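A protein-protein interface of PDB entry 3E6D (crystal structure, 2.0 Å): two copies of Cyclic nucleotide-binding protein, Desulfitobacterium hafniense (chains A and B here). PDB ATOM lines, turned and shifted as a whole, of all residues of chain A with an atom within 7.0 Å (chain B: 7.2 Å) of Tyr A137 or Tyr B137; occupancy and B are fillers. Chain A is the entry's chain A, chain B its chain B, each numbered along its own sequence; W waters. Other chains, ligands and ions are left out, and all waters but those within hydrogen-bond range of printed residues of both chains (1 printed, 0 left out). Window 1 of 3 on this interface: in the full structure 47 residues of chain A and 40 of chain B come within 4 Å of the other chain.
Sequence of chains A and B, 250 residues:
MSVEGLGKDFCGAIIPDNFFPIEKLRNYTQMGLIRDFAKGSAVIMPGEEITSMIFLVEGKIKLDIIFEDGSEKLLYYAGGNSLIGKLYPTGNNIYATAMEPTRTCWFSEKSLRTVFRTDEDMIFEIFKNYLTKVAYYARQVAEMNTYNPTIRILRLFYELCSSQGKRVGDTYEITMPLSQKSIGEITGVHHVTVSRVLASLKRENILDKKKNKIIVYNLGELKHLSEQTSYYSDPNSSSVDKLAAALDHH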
ATOM      1  N   ASN A  18     -11.819  -8.813  12.557  1.00  0.00           N
ATOM      2  CA  ASN A  18     -11.840  -7.838  11.471  1.00  0.00           C
ATOM      3  C   ASN A  18     -10.442  -7.314  11.142  1.00  0.00           C
ATOM      4  O   ASN A  18      -9.807  -6.645  11.958  1.00  0.00           O
ATOM      5  CB  ASN A  18     -12.798  -6.686  11.795  1.00  0.00           C
ATOM      6  N   PHE A  20      -9.705  -5.254   8.654  1.00  0.00           N
ATOM      7  CA  PHE A  20      -9.758  -3.915   8.071  1.00  0.00           C
ATOM      8  C   PHE A  20      -8.804  -3.784   6.890  1.00  0.00           C
ATOM      9  O   PHE A  20      -7.884  -2.970   6.924  1.00  0.00           O
ATOM     10  CB  PHE A  20      -9.393  -2.866   9.120  1.00  0.00           C
ATOM     11  CG  PHE A  20     -10.280  -2.879  10.335  1.00  0.00           C
ATOM     12  CD1 PHE A  20      -9.791  -3.306  11.561  1.00  0.00           C
ATOM     13  CD2 PHE A  20     -11.595  -2.448  10.256  1.00  0.00           C
ATOM     14  CE1 PHE A  20     -10.600  -3.312  12.682  1.00  0.00           C
ATOM     15  CE2 PHE A  20     -12.408  -2.451  11.375  1.00  0.00           C
ATOM     16  CZ  PHE A  20     -11.909  -2.884  12.590  1.00  0.00           C
ATOM     17  N   LEU A  75      -4.335  -8.050  21.821  1.00  0.00           N
ATOM     18  CA  LEU A  75      -4.662  -6.731  21.293  1.00  0.00           C
ATOM     19  C   LEU A  75      -5.560  -6.896  20.073  1.00  0.00           C
ATOM     20  O   LEU A  75      -6.782  -6.790  20.176  1.00  0.00           O
ATOM     21  CB  LEU A  75      -3.396  -5.953  20.932  1.00  0.00           C
ATOM     22  CG  LEU A  75      -3.622  -4.489  20.555  1.00  0.00           C
ATOM     23  CD1 LEU A  75      -3.867  -3.666  21.801  1.00  0.00           C
ATOM     24  CD2 LEU A  75      -2.441  -3.943  19.772  1.00  0.00           C
ATOM     25  N   TYR A  76      -4.956  -7.145  18.916  1.00  0.00           N
ATOM     26  CA  TYR A  76      -5.715  -7.621  17.759  1.00  0.00           C
ATOM     27  C   TYR A  76      -4.920  -8.585  16.900  1.00  0.00           C
ATOM     28  O   TYR A  76      -3.721  -8.777  17.100  1.00  0.00           O
ATOM     29  CB  TYR A  76      -6.284  -6.480  16.897  1.00  0.00           C
ATOM     30  CG  TYR A  76      -5.472  -5.198  16.866  1.00  0.00           C
ATOM     31  CD1 TYR A  76      -5.716  -4.187  17.784  1.00  0.00           C
ATOM     32  CD2 TYR A  76      -4.484  -4.986  15.912  1.00  0.00           C
ATOM     33  CE1 TYR A  76      -5.004  -3.002  17.764  1.00  0.00           C
ATOM     34  CE2 TYR A  76      -3.752  -3.801  15.888  1.00  0.00           C
ATOM     35  CZ  TYR A  76      -4.029  -2.812  16.818  1.00  0.00           C
ATOM     36  OH  TYR A  76      -3.321  -1.638  16.820  1.00  0.00           O
ATOM     37  N   TYR A  77      -5.617  -9.213  15.962  1.00  0.00           N
ATOM     38  CA  TYR A  77      -4.998 -10.109  15.000  1.00  0.00           C
ATOM     39  C   TYR A  77      -5.002  -9.442  13.634  1.00  0.00           C
ATOM     40  O   TYR A  77      -6.062  -9.161  13.081  1.00  0.00           O
ATOM     41  CB  TYR A  77      -5.772 -11.424  14.920  1.00  0.00           C
ATOM     42  CG  TYR A  77      -5.574 -12.348  16.098  1.00  0.00           C
ATOM     43  CD1 TYR A  77      -6.490 -12.387  17.141  1.00  0.00           C
ATOM     44  CD2 TYR A  77      -4.477 -13.195  16.160  1.00  0.00           C
ATOM     45  CE1 TYR A  77      -6.311 -13.239  18.216  1.00  0.00           C
ATOM     46  CE2 TYR A  77      -4.290 -14.047  17.228  1.00  0.00           C
ATOM     47  CZ  TYR A  77      -5.209 -14.068  18.253  1.00  0.00           C
ATOM     48  OH  TYR A  77      -5.021 -14.920  19.318  1.00  0.00           O
ATOM     49  N   ASN A  92       1.276   2.698  23.632  1.00  0.00           N
ATOM     50  CA  ASN A  92       1.012   1.266  23.737  1.00  0.00           C
ATOM     51  C   ASN A  92       2.277   0.449  23.489  1.00  0.00           C
ATOM     52  O   ASN A  92       2.750   0.360  22.355  1.00  0.00           O
ATOM     53  CB  ASN A  92      -0.062   0.835  22.732  1.00  0.00           C
ATOM     54  CG  ASN A  92      -1.464   1.278  23.129  1.00  0.00           C
ATOM     55  OD1 ASN A  92      -1.653   1.975  24.128  1.00  0.00           O
ATOM     56  ND2 ASN A  92      -2.456   0.869  22.343  1.00  0.00           N
ATOM     57  N   THR A 132     -12.858   3.786   9.597  1.00  0.00           N
ATOM     58  CA  THR A 132     -13.556   2.522   9.827  1.00  0.00           C
ATOM     59  C   THR A 132     -13.155   1.857  11.153  1.00  0.00           C
ATOM     60  O   THR A 132     -14.000   1.317  11.867  1.00  0.00           O
ATOM     61  CB  THR A 132     -13.312   1.538   8.670  1.00  0.00           C
ATOM     62  OG1 THR A 132     -13.631   2.172   7.425  1.00  0.00           O
ATOM     63  CG2 THR A 132     -14.165   0.287   8.834  1.00  0.00           C
ATOM     64  N   LYS A 133     -11.867   1.899  11.478  1.00  0.00           N
ATOM     65  CA  LYS A 133     -11.378   1.330  12.730  1.00  0.00           C
ATOM     66  C   LYS A 133     -11.903   2.075  13.957  1.00  0.00           C
ATOM     67  O   LYS A 133     -12.292   1.463  14.955  1.00  0.00           O
ATOM     68  CB  LYS A 133      -9.851   1.325  12.748  1.00  0.00           C
ATOM     69  CG  LYS A 133      -9.227   0.494  11.652  1.00  0.00           C
ATOM     70  CD  LYS A 133      -7.710   0.529  11.761  1.00  0.00           C
ATOM     71  CE  LYS A 133      -7.064  -0.518  10.868  1.00  0.00           C
ATOM     72  NZ  LYS A 133      -5.585  -0.505  10.985  1.00  0.00           N
ATOM     73  N   VAL A 134     -11.911   3.400  13.880  1.00  0.00           N
ATOM     74  CA  VAL A 134     -12.398   4.215  14.985  1.00  0.00           C
ATOM     75  C   VAL A 134     -13.904   4.040  15.151  1.00  0.00           C
ATOM     76  O   VAL A 134     -14.428   4.135  16.256  1.00  0.00           O
ATOM     77  CB  VAL A 134     -12.061   5.704  14.782  1.00  0.00           C
ATOM     78  CG1 VAL A 134     -12.775   6.556  15.819  1.00  0.00           C
ATOM     79  CG2 VAL A 134     -10.551   5.922  14.848  1.00  0.00           C
ATOM     80  N   ALA A 135     -14.595   3.778  14.047  1.00  0.00           N
ATOM     81  CA  ALA A 135     -16.028   3.518  14.102  1.00  0.00           C
ATOM     82  C   ALA A 135     -16.246   2.207  14.838  1.00  0.00           C
ATOM     83  O   ALA A 135     -17.076   2.111  15.743  1.00  0.00           O
ATOM     84  CB  ALA A 135     -16.612   3.443  12.702  1.00  0.00           C
ATOM     85  N   TYR A 136     -15.479   1.201  14.436  1.00  0.00           N
ATOM     86  CA  TYR A 136     -15.540  -0.119  15.044  1.00  0.00           C
ATOM     87  C   TYR A 136     -15.339  -0.064  16.556  1.00  0.00           C
ATOM     88  O   TYR A 136     -16.210  -0.486  17.317  1.00  0.00           O
ATOM     89  CB  TYR A 136     -14.476  -1.022  14.423  1.00  0.00           C
ATOM     90  CG  TYR A 136     -14.528  -2.455  14.893  1.00  0.00           C
ATOM     91  CD1 TYR A 136     -15.557  -3.296  14.487  1.00  0.00           C
ATOM     92  CD2 TYR A 136     -13.544  -2.974  15.723  1.00  0.00           C
ATOM     93  CE1 TYR A 136     -15.612  -4.610  14.902  1.00  0.00           C
ATOM     94  CE2 TYR A 136     -13.588  -4.293  16.143  1.00  0.00           C
ATOM     95  CZ  TYR A 136     -14.628  -5.107  15.728  1.00  0.00           C
ATOM     96  OH  TYR A 136     -14.691  -6.421  16.137  1.00  0.00           O
ATOM     97  N   TYR A 137     -14.191   0.461  16.981  1.00  0.00           N
ATOM     98  CA  TYR A 137     -13.783   0.417  18.387  1.00  0.00           C
ATOM     99  C   TYR A 137     -14.659   1.245  19.322  1.00  0.00           C
ATOM    100  O   TYR A 137     -14.990   0.804  20.420  1.00  0.00           O
ATOM    101  CB  TYR A 137     -12.311   0.814  18.542  1.00  0.00           C
ATOM    102  CG  TYR A 137     -11.352  -0.237  18.022  1.00  0.00           C
ATOM    103  CD1 TYR A 137     -10.614  -0.023  16.869  1.00  0.00           C
ATOM    104  CD2 TYR A 137     -11.207  -1.449  18.678  1.00  0.00           C
ATOM    105  CE1 TYR A 137      -9.752  -0.993  16.381  1.00  0.00           C
ATOM    106  CE2 TYR A 137     -10.346  -2.425  18.205  1.00  0.00           C
ATOM    107  CZ  TYR A 137      -9.620  -2.192  17.057  1.00  0.00           C
ATOM    108  OH  TYR A 137      -8.755  -3.152  16.581  1.00  0.00           O
ATOM    109  N   ALA A 138     -15.030   2.445  18.894  1.00  0.00           N
ATOM    110  CA  ALA A 138     -15.897   3.295  19.700  1.00  0.00           C
ATOM    111  C   ALA A 138     -17.241   2.611  19.915  1.00  0.00           C
ATOM    112  O   ALA A 138     -17.813   2.670  21.002  1.00  0.00           O
ATOM    113  CB  ALA A 138     -16.083   4.648  19.034  1.00  0.00           C
ATOM    114  N   ARG A 139     -17.734   1.953  18.871  1.00  0.00           N
ATOM    115  CA  ARG A 139     -19.013   1.255  18.935  1.00  0.00           C
ATOM    116  C   ARG A 139     -18.997   0.084  19.919  1.00  0.00           C
ATOM    117  O   ARG A 139     -20.006  -0.216  20.560  1.00  0.00           O
ATOM    118  CB  ARG A 139     -19.413   0.750  17.552  1.00  0.00           C
ATOM    119  CG  ARG A 139     -20.600  -0.188  17.584  1.00  0.00           C
ATOM    120  CD  ARG A 139     -20.944  -0.702  16.204  1.00  0.00           C
ATOM    121  NE  ARG A 139     -22.376  -0.946  16.088  1.00  0.00           N
ATOM    122  CZ  ARG A 139     -22.979  -1.354  14.978  1.00  0.00           C
ATOM    123  NH1 ARG A 139     -22.271  -1.574  13.878  1.00  0.00           N
ATOM    124  NH2 ARG A 139     -24.292  -1.544  14.971  1.00  0.00           N
ATOM    125  N   GLN A 140     -17.855  -0.588  20.020  1.00  0.00           N
ATOM    126  CA  GLN A 140     -17.701  -1.692  20.960  1.00  0.00           C
ATOM    127  C   GLN A 140     -17.629  -1.127  22.370  1.00  0.00           C
ATOM    128  O   GLN A 140     -18.344  -1.568  23.270  1.00  0.00           O
ATOM    129  CB  GLN A 140     -16.424  -2.471  20.661  1.00  0.00           C
ATOM    130  CG  GLN A 140     -16.213  -2.800  19.192  1.00  0.00           C
ATOM    131  CD  GLN A 140     -16.866  -4.105  18.771  1.00  0.00           C
ATOM    132  OE1 GLN A 140     -18.075  -4.291  18.921  1.00  0.00           O
ATOM    133  NE2 GLN A 140     -16.064  -5.017  18.229  1.00  0.00           N
ATOM    134  N   VAL A 141     -16.755  -0.140  22.547  1.00  0.00           N
ATOM    135  CA  VAL A 141     -16.564   0.515  23.833  1.00  0.00           C
ATOM    136  C   VAL A 141     -17.801   1.321  24.215  1.00  0.00           C
ATOM    137  O   VAL A 141     -18.140   1.439  25.396  1.00  0.00           O
ATOM    138  CB  VAL A 141     -15.338   1.452  23.805  1.00  0.00           C
ATOM    139  CG1 VAL A 141     -15.139   2.117  25.157  1.00  0.00           C
ATOM    140  CG2 VAL A 141     -14.086   0.682  23.394  1.00  0.00           C
ATOM    141  N   PHE B  20      -8.723  14.472  22.084  1.00  0.00           N
ATOM    142  CA  PHE B  20      -7.790  14.217  20.982  1.00  0.00           C
ATOM    143  C   PHE B  20      -7.617  15.448  20.092  1.00  0.00           C
ATOM    144  O   PHE B  20      -7.925  15.403  18.901  1.00  0.00           O
ATOM    145  CB  PHE B  20      -8.248  13.027  20.129  1.00  0.00           C
ATOM    146  CG  PHE B  20      -8.308  11.727  20.881  1.00  0.00           C
ATOM    147  CD1 PHE B  20      -9.529  11.145  21.186  1.00  0.00           C
ATOM    148  CD2 PHE B  20      -7.148  11.092  21.286  1.00  0.00           C
ATOM    149  CE1 PHE B  20      -9.590   9.949  21.876  1.00  0.00           C
ATOM    150  CE2 PHE B  20      -7.200   9.897  21.980  1.00  0.00           C
ATOM    151  CZ  PHE B  20      -8.423   9.324  22.278  1.00  0.00           C
ATOM    152  N   LEU B  75     -21.581   7.936  22.942  1.00  0.00           N
ATOM    153  CA  LEU B  75     -20.411   7.402  22.255  1.00  0.00           C
ATOM    154  C   LEU B  75     -19.138   8.043  22.794  1.00  0.00           C
ATOM    155  O   LEU B  75     -18.235   7.356  23.268  1.00  0.00           O
ATOM    156  CB  LEU B  75     -20.531   7.648  20.752  1.00  0.00           C
ATOM    157  CG  LEU B  75     -20.246   6.462  19.835  1.00  0.00           C
ATOM    158  CD1 LEU B  75     -20.013   6.951  18.414  1.00  0.00           C
ATOM    159  CD2 LEU B  75     -19.052   5.670  20.330  1.00  0.00           C
ATOM    160  N   TYR B  76     -19.071   9.367  22.697  1.00  0.00           N
ATOM    161  CA  TYR B  76     -18.043  10.157  23.368  1.00  0.00           C
ATOM    162  C   TYR B  76     -18.372  11.641  23.272  1.00  0.00           C
ATOM    163  O   TYR B  76     -19.147  12.055  22.410  1.00  0.00           O
ATOM    164  CB  TYR B  76     -16.635   9.872  22.815  1.00  0.00           C
ATOM    165  CG  TYR B  76     -16.499   9.890  21.302  1.00  0.00           C
ATOM    166  CD1 TYR B  76     -16.398   8.705  20.583  1.00  0.00           C
ATOM    167  CD2 TYR B  76     -16.447  11.088  20.596  1.00  0.00           C
ATOM    168  CE1 TYR B  76     -16.262   8.707  19.201  1.00  0.00           C
ATOM    169  CE2 TYR B  76     -16.313  11.101  19.210  1.00  0.00           C
ATOM    170  CZ  TYR B  76     -16.221   9.906  18.519  1.00  0.00           C
ATOM    171  OH  TYR B  76     -16.088   9.907  17.144  1.00  0.00           O
ATOM    172  N   TYR B  77     -17.804  12.436  24.173  1.00  0.00           N
ATOM    173  CA  TYR B  77     -17.932  13.884  24.080  1.00  0.00           C
ATOM    174  C   TYR B  77     -16.837  14.423  23.167  1.00  0.00           C
ATOM    175  O   TYR B  77     -15.863  13.728  22.874  1.00  0.00           O
ATOM    176  CB  TYR B  77     -17.826  14.536  25.459  1.00  0.00           C
ATOM    177  CG  TYR B  77     -19.030  14.331  26.350  1.00  0.00           C
ATOM    178  CD1 TYR B  77     -19.083  13.269  27.245  1.00  0.00           C
ATOM    179  CD2 TYR B  77     -20.111  15.205  26.306  1.00  0.00           C
ATOM    180  CE1 TYR B  77     -20.177  13.081  28.065  1.00  0.00           C
ATOM    181  CE2 TYR B  77     -21.211  15.024  27.126  1.00  0.00           C
ATOM    182  CZ  TYR B  77     -21.238  13.959  28.004  1.00  0.00           C
ATOM    183  OH  TYR B  77     -22.327  13.763  28.825  1.00  0.00           O
ATOM    184  N   ASN B  92     -22.468   3.225  11.438  1.00  0.00           N
ATOM    185  CA  ASN B  92     -22.836   3.754  12.744  1.00  0.00           C
ATOM    186  C   ASN B  92     -23.805   4.906  12.551  1.00  0.00           C
ATOM    187  O   ASN B  92     -23.510   5.846  11.817  1.00  0.00           O
ATOM    188  CB  ASN B  92     -21.602   4.268  13.494  1.00  0.00           C
ATOM    189  CG  ASN B  92     -20.882   3.176  14.276  1.00  0.00           C
ATOM    190  OD1 ASN B  92     -21.279   2.010  14.265  1.00  0.00           O
ATOM    191  ND2 ASN B  92     -19.811   3.559  14.963  1.00  0.00           N
ATOM    192  N   LEU B 131      -4.361   7.565  14.341  1.00  0.00           N
ATOM    193  CA  LEU B 131      -3.551   6.514  14.944  1.00  0.00           C
ATOM    194  C   LEU B 131      -3.704   6.560  16.459  1.00  0.00           C
ATOM    195  O   LEU B 131      -3.905   5.535  17.102  1.00  0.00           O
ATOM    196  CB  LEU B 131      -2.075   6.676  14.567  1.00  0.00           C
ATOM    197  CG  LEU B 131      -1.600   6.078  13.244  1.00  0.00           C
ATOM    198  CD1 LEU B 131      -0.373   6.820  12.718  1.00  0.00           C
ATOM    199  CD2 LEU B 131      -1.315   4.583  13.396  1.00  0.00           C
ATOM    200  N   THR B 132      -3.599   7.757  17.026  1.00  0.00           N
ATOM    201  CA  THR B 132      -3.722   7.930  18.469  1.00  0.00           C
ATOM    202  C   THR B 132      -5.100   7.483  18.958  1.00  0.00           C
ATOM    203  O   THR B 132      -5.217   6.813  19.988  1.00  0.00           O
ATOM    204  CB  THR B 132      -3.482   9.398  18.888  1.00  0.00           C
ATOM    205  OG1 THR B 132      -2.146   9.783  18.545  1.00  0.00           O
ATOM    206  CG2 THR B 132      -3.679   9.563  20.388  1.00  0.00           C
ATOM    207  N   LYS B 133      -6.137   7.842  18.205  1.00  0.00           N
ATOM    208  CA  LYS B 133      -7.511   7.472  18.538  1.00  0.00           C
ATOM    209  C   LYS B 133      -7.709   5.965  18.546  1.00  0.00           C
ATOM    210  O   LYS B 133      -8.209   5.405  19.520  1.00  0.00           O
ATOM    211  CB  LYS B 133      -8.497   8.130  17.569  1.00  0.00           C
ATOM    212  CG  LYS B 133      -8.765   9.594  17.869  1.00  0.00           C
ATOM    213  CD  LYS B 133      -9.516  10.269  16.739  1.00  0.00           C
ATOM    214  CE  LYS B 133     -10.210  11.524  17.233  1.00  0.00           C
ATOM    215  NZ  LYS B 133     -10.513  12.470  16.122  1.00  0.00           N
ATOM    216  N   VAL B 134      -7.321   5.312  17.457  1.00  0.00           N
ATOM    217  CA  VAL B 134      -7.393   3.858  17.373  1.00  0.00           C
ATOM    218  C   VAL B 134      -6.633   3.165  18.516  1.00  0.00           C
ATOM    219  O   VAL B 134      -7.122   2.198  19.103  1.00  0.00           O
ATOM    220  CB  VAL B 134      -6.833   3.345  16.042  1.00  0.00           C
ATOM    221  CG1 VAL B 134      -6.788   1.840  16.054  1.00  0.00           C
ATOM    222  CG2 VAL B 134      -7.674   3.853  14.877  1.00  0.00           C
ATOM    223  N   ALA B 135      -5.437   3.659  18.823  1.00  0.00           N
ATOM    224  CA  ALA B 135      -4.605   3.065  19.867  1.00  0.00           C
ATOM    225  C   ALA B 135      -5.274   3.134  21.235  1.00  0.00           C
ATOM    226  O   ALA B 135      -5.159   2.207  22.038  1.00  0.00           O
ATOM    227  CB  ALA B 135      -3.234   3.728  19.907  1.00  0.00           C
ATOM    228  N   TYR B 136      -5.966   4.237  21.501  1.00  0.00           N
ATOM    229  CA  TYR B 136      -6.676   4.389  22.765  1.00  0.00           C
ATOM    230  C   TYR B 136      -7.784   3.346  22.886  1.00  0.00           C
ATOM    231  O   TYR B 136      -7.807   2.560  23.832  1.00  0.00           O
ATOM    232  CB  TYR B 136      -7.254   5.800  22.906  1.00  0.00           C
ATOM    233  CG  TYR B 136      -7.949   6.043  24.229  1.00  0.00           C
ATOM    234  CD1 TYR B 136      -7.219   6.155  25.405  1.00  0.00           C
ATOM    235  CD2 TYR B 136      -9.333   6.162  24.303  1.00  0.00           C
ATOM    236  CE1 TYR B 136      -7.844   6.378  26.615  1.00  0.00           C
ATOM    237  CE2 TYR B 136      -9.967   6.384  25.514  1.00  0.00           C
ATOM    238  CZ  TYR B 136      -9.214   6.492  26.664  1.00  0.00           C
ATOM    239  OH  TYR B 136      -9.824   6.715  27.877  1.00  0.00           O
ATOM    240  N   TYR B 137      -8.689   3.331  21.913  1.00  0.00           N
ATOM    241  CA  TYR B 137      -9.816   2.401  21.928  1.00  0.00           C
ATOM    242  C   TYR B 137      -9.383   0.940  21.947  1.00  0.00           C
ATOM    243  O   TYR B 137      -9.937   0.133  22.696  1.00  0.00           O
ATOM    244  CB  TYR B 137     -10.749   2.667  20.749  1.00  0.00           C
ATOM    245  CG  TYR B 137     -11.534   3.941  20.900  1.00  0.00           C
ATOM    246  CD1 TYR B 137     -11.343   5.008  20.030  1.00  0.00           C
ATOM    247  CD2 TYR B 137     -12.454   4.089  21.930  1.00  0.00           C
ATOM    248  CE1 TYR B 137     -12.061   6.184  20.177  1.00  0.00           C
ATOM    249  CE2 TYR B 137     -13.172   5.257  22.085  1.00  0.00           C
ATOM    250  CZ  TYR B 137     -12.972   6.301  21.208  1.00  0.00           C
ATOM    251  OH  TYR B 137     -13.690   7.462  21.365  1.00  0.00           O
ATOM    252  N   ALA B 138      -8.397   0.600  21.122  1.00  0.00           N
ATOM    253  CA  ALA B 138      -7.859  -0.754  21.107  1.00  0.00           C
ATOM    254  C   ALA B 138      -7.378  -1.129  22.505  1.00  0.00           C
ATOM    255  O   ALA B 138      -7.639  -2.228  22.993  1.00  0.00           O
ATOM    256  CB  ALA B 138      -6.716  -0.860  20.107  1.00  0.00           C
ATOM    257  N   ARG B 139      -6.682  -0.197  23.146  1.00  0.00           N
ATOM    258  CA  ARG B 139      -6.130  -0.413  24.477  1.00  0.00           C
ATOM    259  C   ARG B 139      -7.222  -0.699  25.507  1.00  0.00           C
ATOM    260  O   ARG B 139      -7.033  -1.511  26.413  1.00  0.00           O
ATOM    261  CB  ARG B 139      -5.312   0.806  24.900  1.00  0.00           C
ATOM    262  CG  ARG B 139      -4.641   0.687  26.248  1.00  0.00           C
ATOM    263  CD  ARG B 139      -3.797   1.918  26.526  1.00  0.00           C
ATOM    264  NE  ARG B 139      -3.222   1.890  27.865  1.00  0.00           N
ATOM    265  CZ  ARG B 139      -2.077   1.291  28.173  1.00  0.00           C
ATOM    266  NH1 ARG B 139      -1.377   0.667  27.235  1.00  0.00           N
ATOM    267  NH2 ARG B 139      -1.631   1.318  29.421  1.00  0.00           N
ATOM    268  N   GLN B 140      -8.362  -0.027  25.367  1.00  0.00           N
ATOM    269  CA  GLN B 140      -9.487  -0.254  26.267  1.00  0.00           C
ATOM    270  C   GLN B 140     -10.074  -1.641  26.026  1.00  0.00           C
ATOM    271  O   GLN B 140     -10.569  -2.287  26.948  1.00  0.00           O
ATOM    272  CB  GLN B 140     -10.566   0.813  26.075  1.00  0.00           C
ATOM    273  CG  GLN B 140     -10.032   2.217  25.888  1.00  0.00           C
ATOM    274  CD  GLN B 140      -9.018   2.603  26.946  1.00  0.00           C
ATOM    275  OE1 GLN B 140      -9.319   2.609  28.141  1.00  0.00           O
ATOM    276  NE2 GLN B 140      -7.808   2.940  26.511  1.00  0.00           N
ATOM    277  N   VAL B 141     -10.009  -2.094  24.777  1.00  0.00           N
ATOM    278  CA  VAL B 141     -10.486  -3.422  24.407  1.00  0.00           C
ATOM    279  C   VAL B 141      -9.348  -4.443  24.390  1.00  0.00           C
ATOM    280  O   VAL B 141      -8.478  -4.442  25.265  1.00  0.00           O
ATOM    281  CB  VAL B 141     -11.169  -3.408  23.021  1.00  0.00           C
ATOM    282  CG1 VAL B 141     -11.451  -4.829  22.553  1.00  0.00           C
ATOM    283  CG2 VAL B 141     -12.447  -2.583  23.062  1.00  0.00           C
HETATM  284  O   HOH W   1     -20.284   0.340  12.501  1.00  0.00           O
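ND2 of Asn A92 is in hydrogen-bond range of O of Ala B135, at 3.0 Å.
The guanidinium group (NH1) of Arg B139 lies close to the side-chain amide oxygen (OD1) of Asn A92 (3.4 Å).
The backbone carbonyl oxygen of Ala A135 sits at hydrogen-bond distance from the side-chain amide nitrogen of Asn B92, 3.2 Å away.
CE1 of Tyr A76 touches CB of Ala B138, at 3.6 Å.
Val B134 touches Lys A133.
CG2 of Val A134 touches CG2 of Val B134 (3.5 Å).
CB of Tyr A137 touches CB of Tyr B137, at 3.3 Å.
O of Ala A138 touches CD2 of Leu B75, at 3.3 Å.
Asn B92 touches Arg A139.
Val A141 touches Val B141.
Phe A20 touches none of the printed residues of chain B.
Of the printed residues of chain B, Val A134 touches Val B134.
Tyr A137 touches one residue of chain B.
Of the printed residues of chain B, Arg A139 touches Asn B92 (3.4 Å).
Phe B20 touches none of the printed residues of chain A.
Printed residues of chain A within 4 Å of Leu B75: Ala A138 (3.3 Å).
Of the printed residues of chain A, Tyr B137 touches Tyr A137.
The nearest residue of chain B that does not touch Tyr A137 is Val B134 (4.1 Å).
The nearest printed residue of chain A that does not touch Val B134 is Tyr A137 (4.1 Å).
Printed residues of chain A that touch a printed residue of chain B: Tyr A76, Asn A92, Lys A133, Val A134, Ala A135, Tyr A137, Ala A138, Arg A139 and Val A141.
Among the printed residues, no Asp or Glu carboxylate lies within 4 Å of a Lys or Arg side-chain nitrogen of the other chain.
Tyr A76 touches Ala B138, but with the chains exchanged Ala A138 does not touch Tyr B76 (4.1 Å).
Val B134 touches its own counterpart, Val A134.
Tyr B137 touches its own counterpart, Tyr A137.
Val B141 touches its own counterpart, Val A141.
Positions printed for both chains: 20, 75, 76, 77, 92, 132, 133, 134, 135, 136, 137, 138, 139, 140 and 141.
Water W1 bridges the side-chain amide oxygen (OD1) of Asn B92 and the guanidinium group (NH1) of Arg A139.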
